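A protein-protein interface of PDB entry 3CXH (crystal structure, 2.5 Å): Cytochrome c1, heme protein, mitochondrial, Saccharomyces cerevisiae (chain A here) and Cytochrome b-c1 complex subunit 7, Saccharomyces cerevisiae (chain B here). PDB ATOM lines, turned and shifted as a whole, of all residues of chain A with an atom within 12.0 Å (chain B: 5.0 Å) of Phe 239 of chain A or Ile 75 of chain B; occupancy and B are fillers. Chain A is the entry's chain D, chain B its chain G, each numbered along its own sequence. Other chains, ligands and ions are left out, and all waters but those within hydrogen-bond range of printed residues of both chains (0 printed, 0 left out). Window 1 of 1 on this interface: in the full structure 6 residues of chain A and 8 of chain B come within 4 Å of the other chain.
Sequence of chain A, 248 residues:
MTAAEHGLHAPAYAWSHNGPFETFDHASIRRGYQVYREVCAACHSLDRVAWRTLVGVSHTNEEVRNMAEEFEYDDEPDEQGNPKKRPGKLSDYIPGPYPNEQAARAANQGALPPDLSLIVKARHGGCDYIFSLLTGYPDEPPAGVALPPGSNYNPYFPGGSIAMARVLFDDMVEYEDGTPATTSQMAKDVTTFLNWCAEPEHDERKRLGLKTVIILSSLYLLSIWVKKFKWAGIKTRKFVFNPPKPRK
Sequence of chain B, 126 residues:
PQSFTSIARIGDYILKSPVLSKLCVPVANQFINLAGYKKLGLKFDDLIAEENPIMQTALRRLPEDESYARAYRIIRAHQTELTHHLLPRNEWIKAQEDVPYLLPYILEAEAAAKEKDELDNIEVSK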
ATOM      1  N   TRP A 231     -14.793  23.610 -21.815  1.00  0.00           N
ATOM      2  CA  TRP A 231     -14.367  22.251 -22.147  1.00  0.00           C
ATOM      3  C   TRP A 231     -14.513  21.865 -23.623  1.00  0.00           C
ATOM      4  O   TRP A 231     -13.911  20.879 -24.065  1.00  0.00           O
ATOM      5  CB  TRP A 231     -15.149  21.235 -21.312  1.00  0.00           C
ATOM      6  CG  TRP A 231     -14.564  20.937 -19.978  1.00  0.00           C
ATOM      7  CD1 TRP A 231     -14.670  21.693 -18.855  1.00  0.00           C
ATOM      8  CD2 TRP A 231     -13.790  19.787 -19.619  1.00  0.00           C
ATOM      9  NE1 TRP A 231     -14.017  21.085 -17.808  1.00  0.00           N
ATOM     10  CE2 TRP A 231     -13.463  19.914 -18.253  1.00  0.00           C
ATOM     11  CE3 TRP A 231     -13.338  18.665 -20.319  1.00  0.00           C
ATOM     12  CZ2 TRP A 231     -12.700  18.959 -17.568  1.00  0.00           C
ATOM     13  CZ3 TRP A 231     -12.581  17.715 -19.641  1.00  0.00           C
ATOM     14  CH2 TRP A 231     -12.270  17.871 -18.276  1.00  0.00           C
ATOM     15  N   ALA A 232     -15.297  22.633 -24.383  1.00  0.00           N
ATOM     16  CA  ALA A 232     -15.552  22.332 -25.806  1.00  0.00           C
ATOM     17  C   ALA A 232     -14.334  21.963 -26.662  1.00  0.00           C
ATOM     18  O   ALA A 232     -14.432  21.096 -27.528  1.00  0.00           O
ATOM     19  CB  ALA A 232     -16.343  23.461 -26.462  1.00  0.00           C
ATOM     20  N   GLY A 233     -13.195  22.607 -26.423  1.00  0.00           N
ATOM     21  CA  GLY A 233     -11.995  22.301 -27.188  1.00  0.00           C
ATOM     22  C   GLY A 233     -11.482  20.906 -26.882  1.00  0.00           C
ATOM     23  O   GLY A 233     -11.001  20.206 -27.769  1.00  0.00           O
ATOM     24  N   ILE A 234     -11.610  20.485 -25.627  1.00  0.00           N
ATOM     25  CA  ILE A 234     -11.150  19.163 -25.213  1.00  0.00           C
ATOM     26  C   ILE A 234     -12.137  18.084 -25.640  1.00  0.00           C
ATOM     27  O   ILE A 234     -11.731  17.012 -26.091  1.00  0.00           O
ATOM     28  CB  ILE A 234     -10.954  19.090 -23.665  1.00  0.00           C
ATOM     29  CG1 ILE A 234      -9.871  20.070 -23.223  1.00  0.00           C
ATOM     30  CG2 ILE A 234     -10.618  17.668 -23.222  1.00  0.00           C
ATOM     31  CD1 ILE A 234      -8.539  19.865 -23.898  1.00  0.00           C
ATOM     32  N   LYS A 235     -13.429  18.368 -25.489  1.00  0.00           N
ATOM     33  CA  LYS A 235     -14.476  17.412 -25.840  1.00  0.00           C
ATOM     34  C   LYS A 235     -14.470  16.986 -27.301  1.00  0.00           C
ATOM     35  O   LYS A 235     -14.567  15.802 -27.601  1.00  0.00           O
ATOM     36  CB  LYS A 235     -15.854  17.975 -25.486  1.00  0.00           C
ATOM     37  CG  LYS A 235     -16.153  18.056 -23.997  1.00  0.00           C
ATOM     38  CD  LYS A 235     -16.456  16.679 -23.428  1.00  0.00           C
ATOM     39  CE  LYS A 235     -17.044  16.788 -22.030  1.00  0.00           C
ATOM     40  NZ  LYS A 235     -17.573  15.484 -21.530  1.00  0.00           N
ATOM     41  N   THR A 236     -14.318  17.951 -28.199  1.00  0.00           N
ATOM     42  CA  THR A 236     -14.327  17.685 -29.633  1.00  0.00           C
ATOM     43  C   THR A 236     -12.953  17.394 -30.245  1.00  0.00           C
ATOM     44  O   THR A 236     -12.835  17.171 -31.444  1.00  0.00           O
ATOM     45  CB  THR A 236     -14.989  18.859 -30.394  1.00  0.00           C
ATOM     46  OG1 THR A 236     -14.184  20.045 -30.264  1.00  0.00           O
ATOM     47  CG2 THR A 236     -16.390  19.128 -29.827  1.00  0.00           C
ATOM     48  N   ARG A 237     -11.927  17.386 -29.410  1.00  0.00           N
ATOM     49  CA  ARG A 237     -10.545  17.120 -29.820  1.00  0.00           C
ATOM     50  C   ARG A 237     -10.421  15.833 -30.645  1.00  0.00           C
ATOM     51  O   ARG A 237     -11.035  14.815 -30.319  1.00  0.00           O
ATOM     52  CB  ARG A 237      -9.697  17.012 -28.550  1.00  0.00           C
ATOM     53  CG  ARG A 237      -8.200  17.117 -28.696  1.00  0.00           C
ATOM     54  CD  ARG A 237      -7.589  17.443 -27.331  1.00  0.00           C
ATOM     55  NE  ARG A 237      -8.033  16.505 -26.304  1.00  0.00           N
ATOM     56  CZ  ARG A 237      -7.273  16.066 -25.306  1.00  0.00           C
ATOM     57  NH1 ARG A 237      -7.770  15.201 -24.427  1.00  0.00           N
ATOM     58  NH2 ARG A 237      -6.017  16.481 -25.192  1.00  0.00           N
ATOM     59  N   LYS A 238      -9.634  15.884 -31.717  1.00  0.00           N
ATOM     60  CA  LYS A 238      -9.429  14.727 -32.586  1.00  0.00           C
ATOM     61  C   LYS A 238      -7.984  14.235 -32.575  1.00  0.00           C
ATOM     62  O   LYS A 238      -7.048  15.037 -32.624  1.00  0.00           O
ATOM     63  CB  LYS A 238      -9.821  15.062 -34.027  1.00  0.00           C
ATOM     64  CG  LYS A 238     -11.186  14.557 -34.459  1.00  0.00           C
ATOM     65  CD  LYS A 238     -12.314  15.407 -33.923  1.00  0.00           C
ATOM     66  CE  LYS A 238     -13.650  14.948 -34.491  1.00  0.00           C
ATOM     67  NZ  LYS A 238     -14.778  15.802 -34.009  1.00  0.00           N
ATOM     68  N   PHE A 239      -7.819  12.912 -32.559  1.00  0.00           N
ATOM     69  CA  PHE A 239      -6.501  12.273 -32.558  1.00  0.00           C
ATOM     70  C   PHE A 239      -6.325  11.287 -33.718  1.00  0.00           C
ATOM     71  O   PHE A 239      -7.196  10.451 -33.954  1.00  0.00           O
ATOM     72  CB  PHE A 239      -6.296  11.486 -31.263  1.00  0.00           C
ATOM     73  CG  PHE A 239      -6.114  12.337 -30.045  1.00  0.00           C
ATOM     74  CD1 PHE A 239      -7.176  12.576 -29.186  1.00  0.00           C
ATOM     75  CD2 PHE A 239      -4.868  12.863 -29.732  1.00  0.00           C
ATOM     76  CE1 PHE A 239      -6.998  13.328 -28.025  1.00  0.00           C
ATOM     77  CE2 PHE A 239      -4.680  13.610 -28.582  1.00  0.00           C
ATOM     78  CZ  PHE A 239      -5.743  13.846 -27.722  1.00  0.00           C
ATOM     79  N   VAL A 240      -5.194  11.360 -34.422  1.00  0.00           N
ATOM     80  CA  VAL A 240      -4.902  10.421 -35.513  1.00  0.00           C
ATOM     81  C   VAL A 240      -3.497   9.840 -35.310  1.00  0.00           C
ATOM     82  O   VAL A 240      -2.592  10.537 -34.862  1.00  0.00           O
ATOM     83  CB  VAL A 240      -5.000  11.078 -36.923  1.00  0.00           C
ATOM     84  CG1 VAL A 240      -6.276  11.904 -37.042  1.00  0.00           C
ATOM     85  CG2 VAL A 240      -3.780  11.930 -37.216  1.00  0.00           C
ATOM     86  N   PHE A 241      -3.319   8.565 -35.639  1.00  0.00           N
ATOM     87  CA  PHE A 241      -2.029   7.901 -35.486  1.00  0.00           C
ATOM     88  C   PHE A 241      -1.417   7.411 -36.798  1.00  0.00           C
ATOM     89  O   PHE A 241      -2.062   6.693 -37.565  1.00  0.00           O
ATOM     90  CB  PHE A 241      -2.184   6.713 -34.549  1.00  0.00           C
ATOM     91  CG  PHE A 241      -0.902   6.006 -34.244  1.00  0.00           C
ATOM     92  CD1 PHE A 241       0.182   6.703 -33.715  1.00  0.00           C
ATOM     93  CD2 PHE A 241      -0.795   4.634 -34.434  1.00  0.00           C
ATOM     94  CE1 PHE A 241       1.361   6.043 -33.369  1.00  0.00           C
ATOM     95  CE2 PHE A 241       0.380   3.952 -34.095  1.00  0.00           C
ATOM     96  CZ  PHE A 241       1.463   4.662 -33.558  1.00  0.00           C
ATOM     97  N   ASN A 242      -0.163   7.782 -37.034  1.00  0.00           N
ATOM     98  CA  ASN A 242       0.576   7.366 -38.219  1.00  0.00           C
ATOM     99  C   ASN A 242       1.849   6.709 -37.734  1.00  0.00           C
ATOM    100  O   ASN A 242       2.808   7.393 -37.373  1.00  0.00           O
ATOM    101  CB  ASN A 242       0.936   8.559 -39.092  1.00  0.00           C
ATOM    102  CG  ASN A 242      -0.232   9.054 -39.893  1.00  0.00           C
ATOM    103  OD1 ASN A 242      -0.697   8.373 -40.805  1.00  0.00           O
ATOM    104  ND2 ASN A 242      -0.722  10.243 -39.561  1.00  0.00           N
ATOM    105  N   PRO A 243       1.873   5.369 -37.711  1.00  0.00           N
ATOM    106  CA  PRO A 243       3.041   4.611 -37.259  1.00  0.00           C
ATOM    107  C   PRO A 243       4.346   5.180 -37.810  1.00  0.00           C
ATOM    108  O   PRO A 243       4.531   5.302 -39.026  1.00  0.00           O
ATOM    109  CB  PRO A 243       2.761   3.207 -37.790  1.00  0.00           C
ATOM    110  CG  PRO A 243       1.272   3.118 -37.677  1.00  0.00           C
ATOM    111  CD  PRO A 243       0.828   4.463 -38.219  1.00  0.00           C
ATOM    112  N   PRO A 244       5.231   5.618 -36.903  1.00  0.00           N
ATOM    113  CA  PRO A 244       6.534   6.191 -37.249  1.00  0.00           C
ATOM    114  C   PRO A 244       7.389   5.119 -37.891  1.00  0.00           C
ATOM    115  O   PRO A 244       7.327   3.956 -37.486  1.00  0.00           O
ATOM    116  CB  PRO A 244       7.113   6.569 -35.882  1.00  0.00           C
ATOM    117  CG  PRO A 244       5.899   6.800 -35.047  1.00  0.00           C
ATOM    118  CD  PRO A 244       5.007   5.670 -35.450  1.00  0.00           C
ATOM    119  N   ALA B  71       1.020   3.876 -26.582  1.00  0.00           N
ATOM    120  CA  ALA B  71       0.806   5.277 -26.226  1.00  0.00           C
ATOM    121  C   ALA B  71      -0.478   5.814 -26.856  1.00  0.00           C
ATOM    122  O   ALA B  71      -1.304   6.408 -26.165  1.00  0.00           O
ATOM    123  CB  ALA B  71       1.980   6.113 -26.654  1.00  0.00           C
ATOM    124  N   TYR B  72      -0.662   5.551 -28.149  1.00  0.00           N
ATOM    125  CA  TYR B  72      -1.842   6.001 -28.878  1.00  0.00           C
ATOM    126  C   TYR B  72      -3.141   5.377 -28.373  1.00  0.00           C
ATOM    127  O   TYR B  72      -4.167   6.055 -28.254  1.00  0.00           O
ATOM    128  CB  TYR B  72      -1.705   5.703 -30.381  1.00  0.00           C
ATOM    129  CG  TYR B  72      -2.941   6.081 -31.170  1.00  0.00           C
ATOM    130  CD1 TYR B  72      -3.319   7.415 -31.290  1.00  0.00           C
ATOM    131  CD2 TYR B  72      -3.761   5.104 -31.746  1.00  0.00           C
ATOM    132  CE1 TYR B  72      -4.477   7.781 -31.956  1.00  0.00           C
ATOM    133  CE2 TYR B  72      -4.937   5.460 -32.422  1.00  0.00           C
ATOM    134  CZ  TYR B  72      -5.285   6.806 -32.522  1.00  0.00           C
ATOM    135  OH  TYR B  72      -6.419   7.201 -33.204  1.00  0.00           O
ATOM    136  N   ARG B  73      -3.114   4.074 -28.125  1.00  0.00           N
ATOM    137  CA  ARG B  73      -4.311   3.400 -27.658  1.00  0.00           C
ATOM    138  C   ARG B  73      -4.778   4.006 -26.343  1.00  0.00           C
ATOM    139  O   ARG B  73      -5.969   4.270 -26.162  1.00  0.00           O
ATOM    140  CB  ARG B  73      -4.079   1.893 -27.552  1.00  0.00           C
ATOM    141  CG  ARG B  73      -3.784   1.229 -28.912  1.00  0.00           C
ATOM    142  CD  ARG B  73      -3.980  -0.277 -28.847  1.00  0.00           C
ATOM    143  NE  ARG B  73      -3.078  -0.889 -27.880  1.00  0.00           N
ATOM    144  CZ  ARG B  73      -1.824  -1.244 -28.146  1.00  0.00           C
ATOM    145  NH1 ARG B  73      -1.072  -1.776 -27.190  1.00  0.00           N
ATOM    146  NH2 ARG B  73      -1.332  -1.106 -29.373  1.00  0.00           N
ATOM    147  N   ILE B  74      -3.824   4.331 -25.475  1.00  0.00           N
ATOM    148  CA  ILE B  74      -4.144   4.933 -24.186  1.00  0.00           C
ATOM    149  C   ILE B  74      -4.735   6.338 -24.350  1.00  0.00           C
ATOM    150  O   ILE B  74      -5.784   6.644 -23.780  1.00  0.00           O
ATOM    151  CB  ILE B  74      -2.894   4.961 -23.270  1.00  0.00           C
ATOM    152  CG1 ILE B  74      -2.453   3.528 -22.965  1.00  0.00           C
ATOM    153  CG2 ILE B  74      -3.179   5.726 -21.972  1.00  0.00           C
ATOM    154  CD1 ILE B  74      -1.186   3.447 -22.152  1.00  0.00           C
ATOM    155  N   ILE B  75      -4.082   7.187 -25.136  1.00  0.00           N
ATOM    156  CA  ILE B  75      -4.582   8.543 -25.341  1.00  0.00           C
ATOM    157  C   ILE B  75      -5.967   8.521 -25.975  1.00  0.00           C
ATOM    158  O   ILE B  75      -6.866   9.240 -25.551  1.00  0.00           O
ATOM    159  CB  ILE B  75      -3.611   9.389 -26.204  1.00  0.00           C
ATOM    160  CG1 ILE B  75      -2.339   9.690 -25.411  1.00  0.00           C
ATOM    161  CG2 ILE B  75      -4.268  10.704 -26.616  1.00  0.00           C
ATOM    162  CD1 ILE B  75      -1.228  10.255 -26.232  1.00  0.00           C
ATOM    163  N   ARG B  76      -6.137   7.644 -26.956  1.00  0.00           N
ATOM    164  CA  ARG B  76      -7.396   7.488 -27.663  1.00  0.00           C
ATOM    165  C   ARG B  76      -8.468   7.067 -26.659  1.00  0.00           C
ATOM    166  O   ARG B  76      -9.568   7.620 -26.638  1.00  0.00           O
ATOM    167  CB  ARG B  76      -7.219   6.441 -28.769  1.00  0.00           C
ATOM    168  CG  ARG B  76      -8.373   6.268 -29.734  1.00  0.00           C
ATOM    169  CD  ARG B  76      -8.712   4.801 -29.836  1.00  0.00           C
ATOM    170  NE  ARG B  76      -8.269   4.165 -31.072  1.00  0.00           N
ATOM    171  CZ  ARG B  76      -7.762   2.934 -31.158  1.00  0.00           C
ATOM    172  NH1 ARG B  76      -7.415   2.458 -32.337  1.00  0.00           N
ATOM    173  NH2 ARG B  76      -7.544   2.198 -30.077  1.00  0.00           N
ATOM    174  N   ALA B  77      -8.117   6.143 -25.774  1.00  0.00           N
ATOM    175  CA  ALA B  77      -9.060   5.664 -24.763  1.00  0.00           C
ATOM    176  C   ALA B  77      -9.507   6.749 -23.797  1.00  0.00           C
ATOM    177  O   ALA B  77     -10.697   6.867 -23.505  1.00  0.00           O
ATOM    178  CB  ALA B  77      -8.463   4.510 -23.994  1.00  0.00           C
ATOM    179  N   HIS B  78      -8.552   7.517 -23.270  1.00  0.00           N
ATOM    180  CA  HIS B  78      -8.874   8.592 -22.328  1.00  0.00           C
ATOM    181  C   HIS B  78      -9.804   9.620 -22.962  1.00  0.00           C
ATOM    182  O   HIS B  78     -10.721  10.108 -22.311  1.00  0.00           O
ATOM    183  CB  HIS B  78      -7.602   9.291 -21.827  1.00  0.00           C
ATOM    184  CG  HIS B  78      -6.937   8.593 -20.684  1.00  0.00           C
ATOM    185  ND1 HIS B  78      -5.687   8.021 -20.785  1.00  0.00           N
ATOM    186  CD2 HIS B  78      -7.347   8.376 -19.413  1.00  0.00           C
ATOM    187  CE1 HIS B  78      -5.357   7.482 -19.626  1.00  0.00           C
ATOM    188  NE2 HIS B  78      -6.346   7.684 -18.776  1.00  0.00           N
ATOM    189  N   GLN B  79      -9.559   9.950 -24.229  1.00  0.00           N
ATOM    190  CA  GLN B  79     -10.376  10.922 -24.946  1.00  0.00           C
ATOM    191  C   GLN B  79     -11.792  10.408 -25.143  1.00  0.00           C
ATOM    192  O   GLN B  79     -12.765  11.124 -24.891  1.00  0.00           O
ATOM    193  CB  GLN B  79      -9.764  11.252 -26.304  1.00  0.00           C
ATOM    194  CG  GLN B  79     -10.606  12.217 -27.135  1.00  0.00           C
ATOM    195  CD  GLN B  79     -10.755  13.581 -26.487  1.00  0.00           C
ATOM    196  OE1 GLN B  79      -9.785  14.162 -26.010  1.00  0.00           O
ATOM    197  NE2 GLN B  79     -11.969  14.105 -26.481  1.00  0.00           N
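Of the printed residues of chain B, Ile 234 of chain A touches Gln 79 (2.9 Å).
Of the printed residues of chain B, Lys 235 of chain A touches Gln 79 (3.3 Å).
Printed residues of chain B within 4 Å of Arg 237 of chain A: Gln 79 (2.8 Å).
Phe 239 of chain A touches just these residues of chain B: Tyr 72 (3.4 Å), Ile 75 (3.5 Å) and Gln 79 (3.5 Å).
Of the printed residues of chain B, Phe 241 of chain A touches Tyr 72.
Pro 243 of chain A touches none of the printed residues of chain B.
No residue of chain A comes within 4 Å of Ala 71 of chain B.
No residue of chain A comes within 4 Å of Ile 74 of chain B.
Of chain A, only Phe 239 (3.5 Å) comes within 4 Å of Ile 75 of chain B.
Arg 76 of chain B touches none of the printed residues of chain A.
No residue of chain A comes within 4 Å of Ala 77 of chain B.
His 78 of chain B touches none of the printed residues of chain A.
The nearest printed residue of chain B that does not touch Phe 239 of chain A is Arg 76 of chain B (5.3 Å).
The nearest residue of chain A that does not touch Ile 75 of chain B is Arg 237 of chain A (6.1 Å).
The backbone carbonyl oxygen (O) of Lys 235 of chain A is in hydrogen-bond range of the side-chain amide nitrogen (NE2) of Gln 79 of chain B, at 3.3 Å.
The guanidinium group (NH1) of Arg 237 of chain A sits at hydrogen-bond distance from the side-chain amide oxygen (OE1) of Gln 79 of chain B (2.8 Å).
The side-chain hydroxyl (OH) of Tyr 72 of chain B sits at hydrogen-bond distance from the backbone carbonyl oxygen (O) of Phe 239 of chain A, at 3.4 Å.
O of Ile 234 of chain A sits at hydrogen-bond distance from NE2 of Gln 79 of chain B (2.9 Å).
Ile 75 of chain B touches Phe 239 of chain A.
Phe 239 of chain A touches Gln 79 of chain B.
Tyr 72 of chain B touches Phe 241 of chain A.
Of the 9 printed residues of chain B, 3 touch a printed residue of chain A.
Printed residues of chain A that touch a printed residue of chain B: Ile 234, Lys 235, Arg 237, Phe 239 and Phe 241.
Hydrophobic or aromatic side chains of chain A that line the printed part of chain B: Phe 239 and Phe 241.
Among the printed residues, 7 pairs touch across the chains.
Among the printed residues, no Asp or Glu carboxylate lies within 4 Å of a Lys or Arg side-chain nitrogen of the other chain.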
